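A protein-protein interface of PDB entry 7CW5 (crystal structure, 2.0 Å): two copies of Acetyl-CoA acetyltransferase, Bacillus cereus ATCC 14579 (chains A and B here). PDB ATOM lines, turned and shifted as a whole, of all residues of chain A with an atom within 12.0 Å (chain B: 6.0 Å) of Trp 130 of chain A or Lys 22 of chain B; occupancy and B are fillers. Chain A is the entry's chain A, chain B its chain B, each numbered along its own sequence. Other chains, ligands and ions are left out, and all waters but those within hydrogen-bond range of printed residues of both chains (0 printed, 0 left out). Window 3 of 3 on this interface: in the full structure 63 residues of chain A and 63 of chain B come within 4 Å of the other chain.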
ATOM      1  N   ILE A 124      29.802   0.217  -7.635  1.00  0.00           N
ATOM      2  CA  ILE A 124      30.064   1.458  -6.875  1.00  0.00           C
ATOM      3  C   ILE A 124      28.795   1.929  -6.197  1.00  0.00           C
ATOM      4  O   ILE A 124      27.653   1.622  -6.660  1.00  0.00           O
ATOM      5  CB  ILE A 124      30.709   2.552  -7.750  1.00  0.00           C
ATOM      6  CG1 ILE A 124      29.739   3.166  -8.758  1.00  0.00           C
ATOM      7  CG2 ILE A 124      31.970   2.017  -8.426  1.00  0.00           C
ATOM      8  CD1 ILE A 124      30.264   4.435  -9.384  1.00  0.00           C
ATOM      9  N   LEU A 125      29.031   2.739  -5.175  1.00  0.00           N
ATOM     10  CA  LEU A 125      27.988   3.431  -4.406  1.00  0.00           C
ATOM     11  C   LEU A 125      28.323   4.917  -4.473  1.00  0.00           C
ATOM     12  O   LEU A 125      29.354   5.325  -3.889  1.00  0.00           O
ATOM     13  CB  LEU A 125      28.008   2.933  -2.955  1.00  0.00           C
ATOM     14  CG  LEU A 125      27.610   1.481  -2.726  1.00  0.00           C
ATOM     15  CD1 LEU A 125      27.886   1.076  -1.291  1.00  0.00           C
ATOM     16  CD2 LEU A 125      26.151   1.245  -3.084  1.00  0.00           C
ATOM     17  N   ARG A 126      27.526   5.676  -5.211  1.00  0.00           N
ATOM     18  CA  ARG A 126      27.557   7.157  -5.169  1.00  0.00           C
ATOM     19  C   ARG A 126      26.616   7.541  -4.028  1.00  0.00           C
ATOM     20  O   ARG A 126      25.582   6.894  -3.894  1.00  0.00           O
ATOM     21  CB  ARG A 126      27.077   7.764  -6.486  1.00  0.00           C
ATOM     22  CG  ARG A 126      27.657   7.170  -7.766  1.00  0.00           C
ATOM     23  CD  ARG A 126      27.106   8.001  -8.923  1.00  0.00           C
ATOM     24  NE  ARG A 126      27.133   7.404 -10.264  1.00  0.00           N
ATOM     25  CZ  ARG A 126      28.183   7.424 -11.064  1.00  0.00           C
ATOM     26  NH1 ARG A 126      29.301   7.968 -10.647  1.00  0.00           N
ATOM     27  NH2 ARG A 126      28.136   6.881 -12.263  1.00  0.00           N
ATOM     28  N   GLY A 127      26.922   8.551  -3.235  1.00  0.00           N
ATOM     29  CA  GLY A 127      25.982   8.985  -2.183  1.00  0.00           C
ATOM     30  C   GLY A 127      26.330   8.446  -0.802  1.00  0.00           C
ATOM     31  O   GLY A 127      26.025   9.171   0.167  1.00  0.00           O
ATOM     32  N   ALA A 128      26.984   7.273  -0.695  1.00  0.00           N
ATOM     33  CA  ALA A 128      27.425   6.637   0.577  1.00  0.00           C
ATOM     34  C   ALA A 128      28.466   7.488   1.327  1.00  0.00           C
ATOM     35  O   ALA A 128      28.499   7.428   2.573  1.00  0.00           O
ATOM     36  CB  ALA A 128      27.968   5.254   0.345  1.00  0.00           C
ATOM     37  N   ARG A 129      29.286   8.268   0.615  1.00  0.00           N
ATOM     38  CA  ARG A 129      30.369   9.071   1.219  1.00  0.00           C
ATOM     39  C   ARG A 129      29.761  10.165   2.100  1.00  0.00           C
ATOM     40  O   ARG A 129      30.230  10.335   3.245  1.00  0.00           O
ATOM     41  CB  ARG A 129      31.281   9.723   0.171  1.00  0.00           C
ATOM     42  CG  ARG A 129      32.480  10.403   0.821  1.00  0.00           C
ATOM     43  CD  ARG A 129      33.430  11.056  -0.149  1.00  0.00           C
ATOM     44  NE  ARG A 129      33.976  10.054  -1.008  1.00  0.00           N
ATOM     45  CZ  ARG A 129      34.940   9.187  -0.659  1.00  0.00           C
ATOM     46  NH1 ARG A 129      35.504   9.263   0.527  1.00  0.00           N
ATOM     47  NH2 ARG A 129      35.341   8.243  -1.508  1.00  0.00           N
ATOM     48  N   TRP A 130      28.763  10.884   1.590  1.00  0.00           N
ATOM     49  CA  TRP A 130      28.164  12.055   2.298  1.00  0.00           C
ATOM     50  C   TRP A 130      26.796  11.671   2.858  1.00  0.00           C
ATOM     51  O   TRP A 130      26.280  12.423   3.730  1.00  0.00           O
ATOM     52  CB  TRP A 130      28.124  13.303   1.407  1.00  0.00           C
ATOM     53  CG  TRP A 130      29.494  13.693   0.943  1.00  0.00           C
ATOM     54  CD1 TRP A 130      29.944  13.727  -0.349  1.00  0.00           C
ATOM     55  CD2 TRP A 130      30.623  14.029   1.777  1.00  0.00           C
ATOM     56  NE1 TRP A 130      31.269  14.067  -0.370  1.00  0.00           N
ATOM     57  CE2 TRP A 130      31.711  14.262   0.913  1.00  0.00           C
ATOM     58  CE3 TRP A 130      30.817  14.156   3.164  1.00  0.00           C
ATOM     59  CZ2 TRP A 130      32.968  14.618   1.399  1.00  0.00           C
ATOM     60  CZ3 TRP A 130      32.061  14.485   3.636  1.00  0.00           C
ATOM     61  CH2 TRP A 130      33.122  14.725   2.764  1.00  0.00           C
ATOM     62  N   GLY A 131      26.299  10.500   2.452  1.00  0.00           N
ATOM     63  CA  GLY A 131      25.171   9.819   3.112  1.00  0.00           C
ATOM     64  C   GLY A 131      23.915   9.898   2.264  1.00  0.00           C
ATOM     65  O   GLY A 131      23.622  10.983   1.741  1.00  0.00           O
ATOM     66  N   TYR A 132      23.160   8.804   2.195  1.00  0.00           N
ATOM     67  CA  TYR A 132      21.884   8.743   1.448  1.00  0.00           C
ATOM     68  C   TYR A 132      20.778   9.475   2.204  1.00  0.00           C
ATOM     69  O   TYR A 132      19.827   9.899   1.550  1.00  0.00           O
ATOM     70  CB  TYR A 132      21.459   7.305   1.246  1.00  0.00           C
ATOM     71  CG  TYR A 132      22.460   6.451   0.516  1.00  0.00           C
ATOM     72  CD1 TYR A 132      22.924   6.809  -0.730  1.00  0.00           C
ATOM     73  CD2 TYR A 132      22.902   5.272   1.073  1.00  0.00           C
ATOM     74  CE1 TYR A 132      23.797   5.989  -1.423  1.00  0.00           C
ATOM     75  CE2 TYR A 132      23.782   4.449   0.400  1.00  0.00           C
ATOM     76  CZ  TYR A 132      24.233   4.812  -0.849  1.00  0.00           C
ATOM     77  OH  TYR A 132      25.088   3.971  -1.501  1.00  0.00           O
ATOM     78  N   ARG A 133      20.872   9.550   3.529  1.00  0.00           N
ATOM     79  CA  ARG A 133      19.856  10.173   4.416  1.00  0.00           C
ATOM     80  C   ARG A 133      18.580   9.317   4.435  1.00  0.00           C
ATOM     81  O   ARG A 133      18.308   8.707   5.477  1.00  0.00           O
ATOM     82  CB  ARG A 133      19.547  11.617   4.000  1.00  0.00           C
ATOM     83  CG  ARG A 133      18.421  12.215   4.834  1.00  0.00           C
ATOM     84  CD  ARG A 133      18.218  13.722   4.744  1.00  0.00           C
ATOM     85  NE  ARG A 133      17.362  14.215   5.823  1.00  0.00           N
ATOM     86  CZ  ARG A 133      16.040  14.365   5.755  1.00  0.00           C
ATOM     87  NH1 ARG A 133      15.380  14.055   4.650  1.00  0.00           N
ATOM     88  NH2 ARG A 133      15.377  14.832   6.802  1.00  0.00           N
ATOM     89  N   MET A 134      17.818   9.256   3.337  1.00  0.00           N
ATOM     90  CA  MET A 134      16.645   8.352   3.228  1.00  0.00           C
ATOM     91  C   MET A 134      16.305   8.093   1.766  1.00  0.00           C
ATOM     92  O   MET A 134      16.689   8.864   0.926  1.00  0.00           O
ATOM     93  CB  MET A 134      15.403   8.895   3.965  1.00  0.00           C
ATOM     94  CG  MET A 134      14.797  10.132   3.380  1.00  0.00           C
ATOM     95  SD  MET A 134      13.235  10.561   4.206  1.00  0.00           S
ATOM     96  CE  MET A 134      13.780  11.092   5.824  1.00  0.00           C
ATOM     97  N   GLY A 135      15.593   7.004   1.507  1.00  0.00           N
ATOM     98  CA  GLY A 135      15.152   6.616   0.163  1.00  0.00           C
ATOM     99  C   GLY A 135      16.162   5.690  -0.470  1.00  0.00           C
ATOM    100  O   GLY A 135      17.310   5.695  -0.056  1.00  0.00           O
ATOM    101  N   ASN A 137      18.581   3.954  -3.345  1.00  0.00           N
ATOM    102  CA  ASN A 137      19.588   4.506  -4.277  1.00  0.00           C
ATOM    103  C   ASN A 137      20.044   3.353  -5.165  1.00  0.00           C
ATOM    104  O   ASN A 137      19.429   2.301  -5.074  1.00  0.00           O
ATOM    105  CB  ASN A 137      20.704   5.196  -3.504  1.00  0.00           C
ATOM    106  CG  ASN A 137      21.153   6.431  -4.241  1.00  0.00           C
ATOM    107  OD1 ASN A 137      21.728   6.336  -5.337  1.00  0.00           O
ATOM    108  ND2 ASN A 137      20.819   7.575  -3.668  1.00  0.00           N
ATOM    109  N   LYS B  16      38.569  22.388  -0.277  1.00  0.00           N
ATOM    110  CA  LYS B  16      38.796  21.337   0.743  1.00  0.00           C
ATOM    111  C   LYS B  16      37.878  20.156   0.454  1.00  0.00           C
ATOM    112  O   LYS B  16      36.807  20.327  -0.172  1.00  0.00           O
ATOM    113  CB  LYS B  16      38.534  21.811   2.170  1.00  0.00           C
ATOM    114  CG  LYS B  16      39.459  22.929   2.621  1.00  0.00           C
ATOM    115  CD  LYS B  16      39.336  23.228   4.088  1.00  0.00           C
ATOM    116  CE  LYS B  16      40.086  22.218   4.930  1.00  0.00           C
ATOM    117  NZ  LYS B  16      40.243  22.745   6.302  1.00  0.00           N
ATOM    118  N   PHE B  17      38.266  19.011   0.973  1.00  0.00           N
ATOM    119  CA  PHE B  17      37.488  17.748   0.900  1.00  0.00           C
ATOM    120  C   PHE B  17      36.125  17.988   1.550  1.00  0.00           C
ATOM    121  O   PHE B  17      36.107  18.402   2.693  1.00  0.00           O
ATOM    122  CB  PHE B  17      38.270  16.679   1.650  1.00  0.00           C
ATOM    123  CG  PHE B  17      37.644  15.324   1.620  1.00  0.00           C
ATOM    124  CD1 PHE B  17      37.583  14.611   0.434  1.00  0.00           C
ATOM    125  CD2 PHE B  17      37.111  14.770   2.770  1.00  0.00           C
ATOM    126  CE1 PHE B  17      37.046  13.334   0.411  1.00  0.00           C
ATOM    127  CE2 PHE B  17      36.573  13.496   2.737  1.00  0.00           C
ATOM    128  CZ  PHE B  17      36.539  12.783   1.563  1.00  0.00           C
ATOM    129  N   GLY B  18      35.018  17.773   0.838  1.00  0.00           N
ATOM    130  CA  GLY B  18      33.682  18.046   1.395  1.00  0.00           C
ATOM    131  C   GLY B  18      33.429  19.541   1.533  1.00  0.00           C
ATOM    132  O   GLY B  18      32.484  19.891   2.192  1.00  0.00           O
ATOM    133  N   GLY B  19      34.207  20.393   0.853  1.00  0.00           N
ATOM    134  CA  GLY B  19      34.190  21.857   1.044  1.00  0.00           C
ATOM    135  C   GLY B  19      33.515  22.604  -0.087  1.00  0.00           C
ATOM    136  O   GLY B  19      32.494  22.097  -0.651  1.00  0.00           O
ATOM    137  N   SER B  20      34.086  23.759  -0.432  1.00  0.00           N
ATOM    138  CA  SER B  20      33.457  24.816  -1.265  1.00  0.00           C
ATOM    139  C   SER B  20      33.142  24.311  -2.682  1.00  0.00           C
ATOM    140  O   SER B  20      32.208  24.834  -3.274  1.00  0.00           O
ATOM    141  CB  SER B  20      34.322  26.053  -1.290  1.00  0.00           C
ATOM    142  OG  SER B  20      35.576  25.808  -1.908  1.00  0.00           O
ATOM    143  N   LEU B  21      33.870  23.329  -3.215  1.00  0.00           N
ATOM    144  CA  LEU B  21      33.618  22.778  -4.583  1.00  0.00           C
ATOM    145  C   LEU B  21      33.020  21.383  -4.516  1.00  0.00           C
ATOM    146  O   LEU B  21      33.011  20.712  -5.566  1.00  0.00           O
ATOM    147  CB  LEU B  21      34.918  22.745  -5.399  1.00  0.00           C
ATOM    148  CG  LEU B  21      35.670  24.071  -5.476  1.00  0.00           C
ATOM    149  CD1 LEU B  21      36.968  23.915  -6.263  1.00  0.00           C
ATOM    150  CD2 LEU B  21      34.782  25.154  -6.083  1.00  0.00           C
ATOM    151  N   LYS B  22      32.521  20.981  -3.343  1.00  0.00           N
ATOM    152  CA  LYS B  22      31.871  19.671  -3.081  1.00  0.00           C
ATOM    153  C   LYS B  22      30.885  19.316  -4.204  1.00  0.00           C
ATOM    154  O   LYS B  22      30.857  18.140  -4.613  1.00  0.00           O
ATOM    155  CB  LYS B  22      31.132  19.734  -1.739  1.00  0.00           C
ATOM    156  CG  LYS B  22      30.385  18.478  -1.333  1.00  0.00           C
ATOM    157  CD  LYS B  22      29.624  18.634  -0.025  1.00  0.00           C
ATOM    158  CE  LYS B  22      28.809  17.402   0.336  1.00  0.00           C
ATOM    159  NZ  LYS B  22      28.544  17.330   1.798  1.00  0.00           N
ATOM    160  N   ASP B  23      30.071  20.277  -4.664  1.00  0.00           N
ATOM    161  CA  ASP B  23      28.909  20.006  -5.552  1.00  0.00           C
ATOM    162  C   ASP B  23      29.334  20.127  -7.019  1.00  0.00           C
ATOM    163  O   ASP B  23      28.441  20.071  -7.901  1.00  0.00           O
ATOM    164  CB  ASP B  23      27.723  20.927  -5.248  1.00  0.00           C
ATOM    165  CG  ASP B  23      27.350  21.032  -3.767  1.00  0.00           C
ATOM    166  OD1 ASP B  23      27.284  20.002  -3.102  1.00  0.00           O
ATOM    167  OD2 ASP B  23      27.149  22.157  -3.298  1.00  0.00           O
ATOM    168  N   VAL B  24      30.629  20.260  -7.313  1.00  0.00           N
ATOM    169  CA  VAL B  24      31.101  20.415  -8.720  1.00  0.00           C
ATOM    170  C   VAL B  24      31.856  19.142  -9.121  1.00  0.00           C
ATOM    171  O   VAL B  24      32.790  18.727  -8.415  1.00  0.00           O
ATOM    172  CB  VAL B  24      31.958  21.675  -8.889  1.00  0.00           C
ATOM    173  CG1 VAL B  24      32.251  21.955 -10.360  1.00  0.00           C
ATOM    174  CG2 VAL B  24      31.300  22.891  -8.232  1.00  0.00           C
ATOM    175  N   LYS B  25      31.499  18.568 -10.253  1.00  0.00           N
ATOM    176  CA  LYS B  25      32.180  17.348 -10.740  1.00  0.00           C
ATOM    177  C   LYS B  25      33.606  17.716 -11.188  1.00  0.00           C
ATOM    178  O   LYS B  25      33.792  18.847 -11.687  1.00  0.00           O
ATOM    179  CB  LYS B  25      31.338  16.746 -11.862  1.00  0.00           C
ATOM    180  CG  LYS B  25      29.929  16.339 -11.444  1.00  0.00           C
ATOM    181  CD  LYS B  25      29.031  15.918 -12.601  1.00  0.00           C
ATOM    182  CE  LYS B  25      29.785  15.250 -13.729  1.00  0.00           C
ATOM    183  NZ  LYS B  25      28.949  14.261 -14.441  1.00  0.00           N
ATOM    184  N   SER B 117      38.117  15.585  -8.323  1.00  0.00           N
ATOM    185  CA  SER B 117      37.129  15.931  -7.266  1.00  0.00           C
ATOM    186  C   SER B 117      37.166  14.785  -6.273  1.00  0.00           C
ATOM    187  O   SER B 117      36.459  13.781  -6.464  1.00  0.00           O
ATOM    188  CB  SER B 117      35.749  16.221  -7.814  1.00  0.00           C
ATOM    189  OG  SER B 117      34.796  16.296  -6.764  1.00  0.00           O
ATOM    190  N   SER B 119      36.328  14.852  -3.270  1.00  0.00           N
ATOM    191  CA  SER B 119      34.999  14.955  -2.625  1.00  0.00           C
ATOM    192  C   SER B 119      34.010  13.967  -3.251  1.00  0.00           C
ATOM    193  O   SER B 119      33.165  13.454  -2.516  1.00  0.00           O
ATOM    194  CB  SER B 119      34.418  16.365  -2.701  1.00  0.00           C
ATOM    195  OG  SER B 119      35.124  17.257  -1.868  1.00  0.00           O
ATOM    196  N   ASN B 120      34.011  13.818  -4.570  1.00  0.00           N
ATOM    197  CA  ASN B 120      32.911  13.111  -5.273  1.00  0.00           C
ATOM    198  C   ASN B 120      33.339  11.683  -5.622  1.00  0.00           C
ATOM    199  O   ASN B 120      32.551  11.006  -6.258  1.00  0.00           O
ATOM    200  CB  ASN B 120      32.399  13.864  -6.489  1.00  0.00           C
ATOM    201  CG  ASN B 120      31.560  15.041  -6.068  1.00  0.00           C
ATOM    202  OD1 ASN B 120      30.602  14.879  -5.325  1.00  0.00           O
ATOM    203  ND2 ASN B 120      31.990  16.234  -6.414  1.00  0.00           N
ATOM    204  N   ILE B 204      28.679  28.345  -8.819  1.00  0.00           N
ATOM    205  CA  ILE B 204      27.879  27.122  -8.532  1.00  0.00           C
ATOM    206  C   ILE B 204      26.422  27.554  -8.508  1.00  0.00           C
ATOM    207  O   ILE B 204      26.039  28.229  -7.558  1.00  0.00           O
ATOM    208  CB  ILE B 204      28.352  26.454  -7.227  1.00  0.00           C
ATOM    209  CG1 ILE B 204      29.863  26.183  -7.260  1.00  0.00           C
ATOM    210  CG2 ILE B 204      27.558  25.188  -6.953  1.00  0.00           C
ATOM    211  CD1 ILE B 204      30.500  25.982  -5.900  1.00  0.00           C
ATOM    212  N   ASP B 252      39.824  19.295  -4.279  1.00  0.00           N
ATOM    213  CA  ASP B 252      39.061  19.412  -5.541  1.00  0.00           C
ATOM    214  C   ASP B 252      39.706  20.544  -6.330  1.00  0.00           C
ATOM    215  O   ASP B 252      40.008  21.603  -5.723  1.00  0.00           O
ATOM    216  CB  ASP B 252      37.572  19.677  -5.302  1.00  0.00           C
ATOM    217  CG  ASP B 252      36.883  18.692  -4.368  1.00  0.00           C
ATOM    218  OD1 ASP B 252      37.286  17.477  -4.359  1.00  0.00           O
ATOM    219  OD2 ASP B 252      35.924  19.139  -3.666  1.00  0.00           O
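OG of Ser 119 of chain B is in hydrogen-bond range of N of Gly 18 of chain B. ND2 of Asn 120 of chain B lies within hydrogen-bond range of O of Lys 22 of chain B, at 2.9 Å. The side-chain hydroxyl (OG) of Ser 119 of chain B is in hydrogen-bond range of the side-chain carboxylate (OD2) of Asp 252 of chain B, at 2.7 Å.
The indole nitrogen of Trp 130 of chain A is in hydrogen-bond range of the backbone carbonyl oxygen of Ser 119 of chain B (2.9 Å).
Arg 129 of chain A touches Phe 17 of chain B (NH1 to CZ, 3.8 Å). Ser 119 of chain B touches Arg 129 of chain A (O to CD, 3.4 Å). Trp 130 of chain A touches Phe 17 of chain B. Gly 18 of chain B touches Trp 130 of chain A (CA to CZ2, 3.5 Å). Trp 130 of chain A touches Lys 22 of chain B (CG to CE, 3.8 Å).
Printed residues of chain A that touch a printed residue of chain B: Arg 129 and Trp 130. Hydrophobic or aromatic side chains of chain A within 4 Å of the printed part of chain B: Trp 130. Among the printed residues, no Asp or Glu carboxylate lies within 4 Å of a Lys or Arg side-chain nitrogen of the other chain.
Trp 130 of chain A touches just these residues of chain B: Phe 17 (3.7 Å), Gly 18 (3.5 Å), Lys 22 (3.8 Å) and Ser 119 (2.9 Å). Of chain A, only Trp 130 (3.8 Å) comes within 4 Å of Lys 22 of chain B. Phe 17 of chain B touches two residues of chain A. Of the printed residues of chain A, Gly 18 of chain B touches Trp 130 (3.5 Å). No residue of chain A comes within 4 Å of Ser 20 of chain B. No residue of chain A comes within 4 Å of Leu 21 of chain B. No residue of chain A comes within 4 Å of Asp 23 of chain B. No residue of chain A comes within 4 Å of Val 24 of chain B. No residue of chain A comes within 4 Å of Asn 120 of chain B. No residue of chain A comes within 4 Å of Asp 252 of chain B. Printed residues of chain B within 4 Å of Arg 129 of chain A: Phe 17 and Ser 119. Lys 16 of chain B touches none of the printed residues of chain A. Arg 126 of chain A touches none of the printed residues of chain B. The nearest printed residue of chain B that does not touch Arg 129 of chain A is Asn 120 of chain B (4.9 Å).
No position is printed for both chains.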
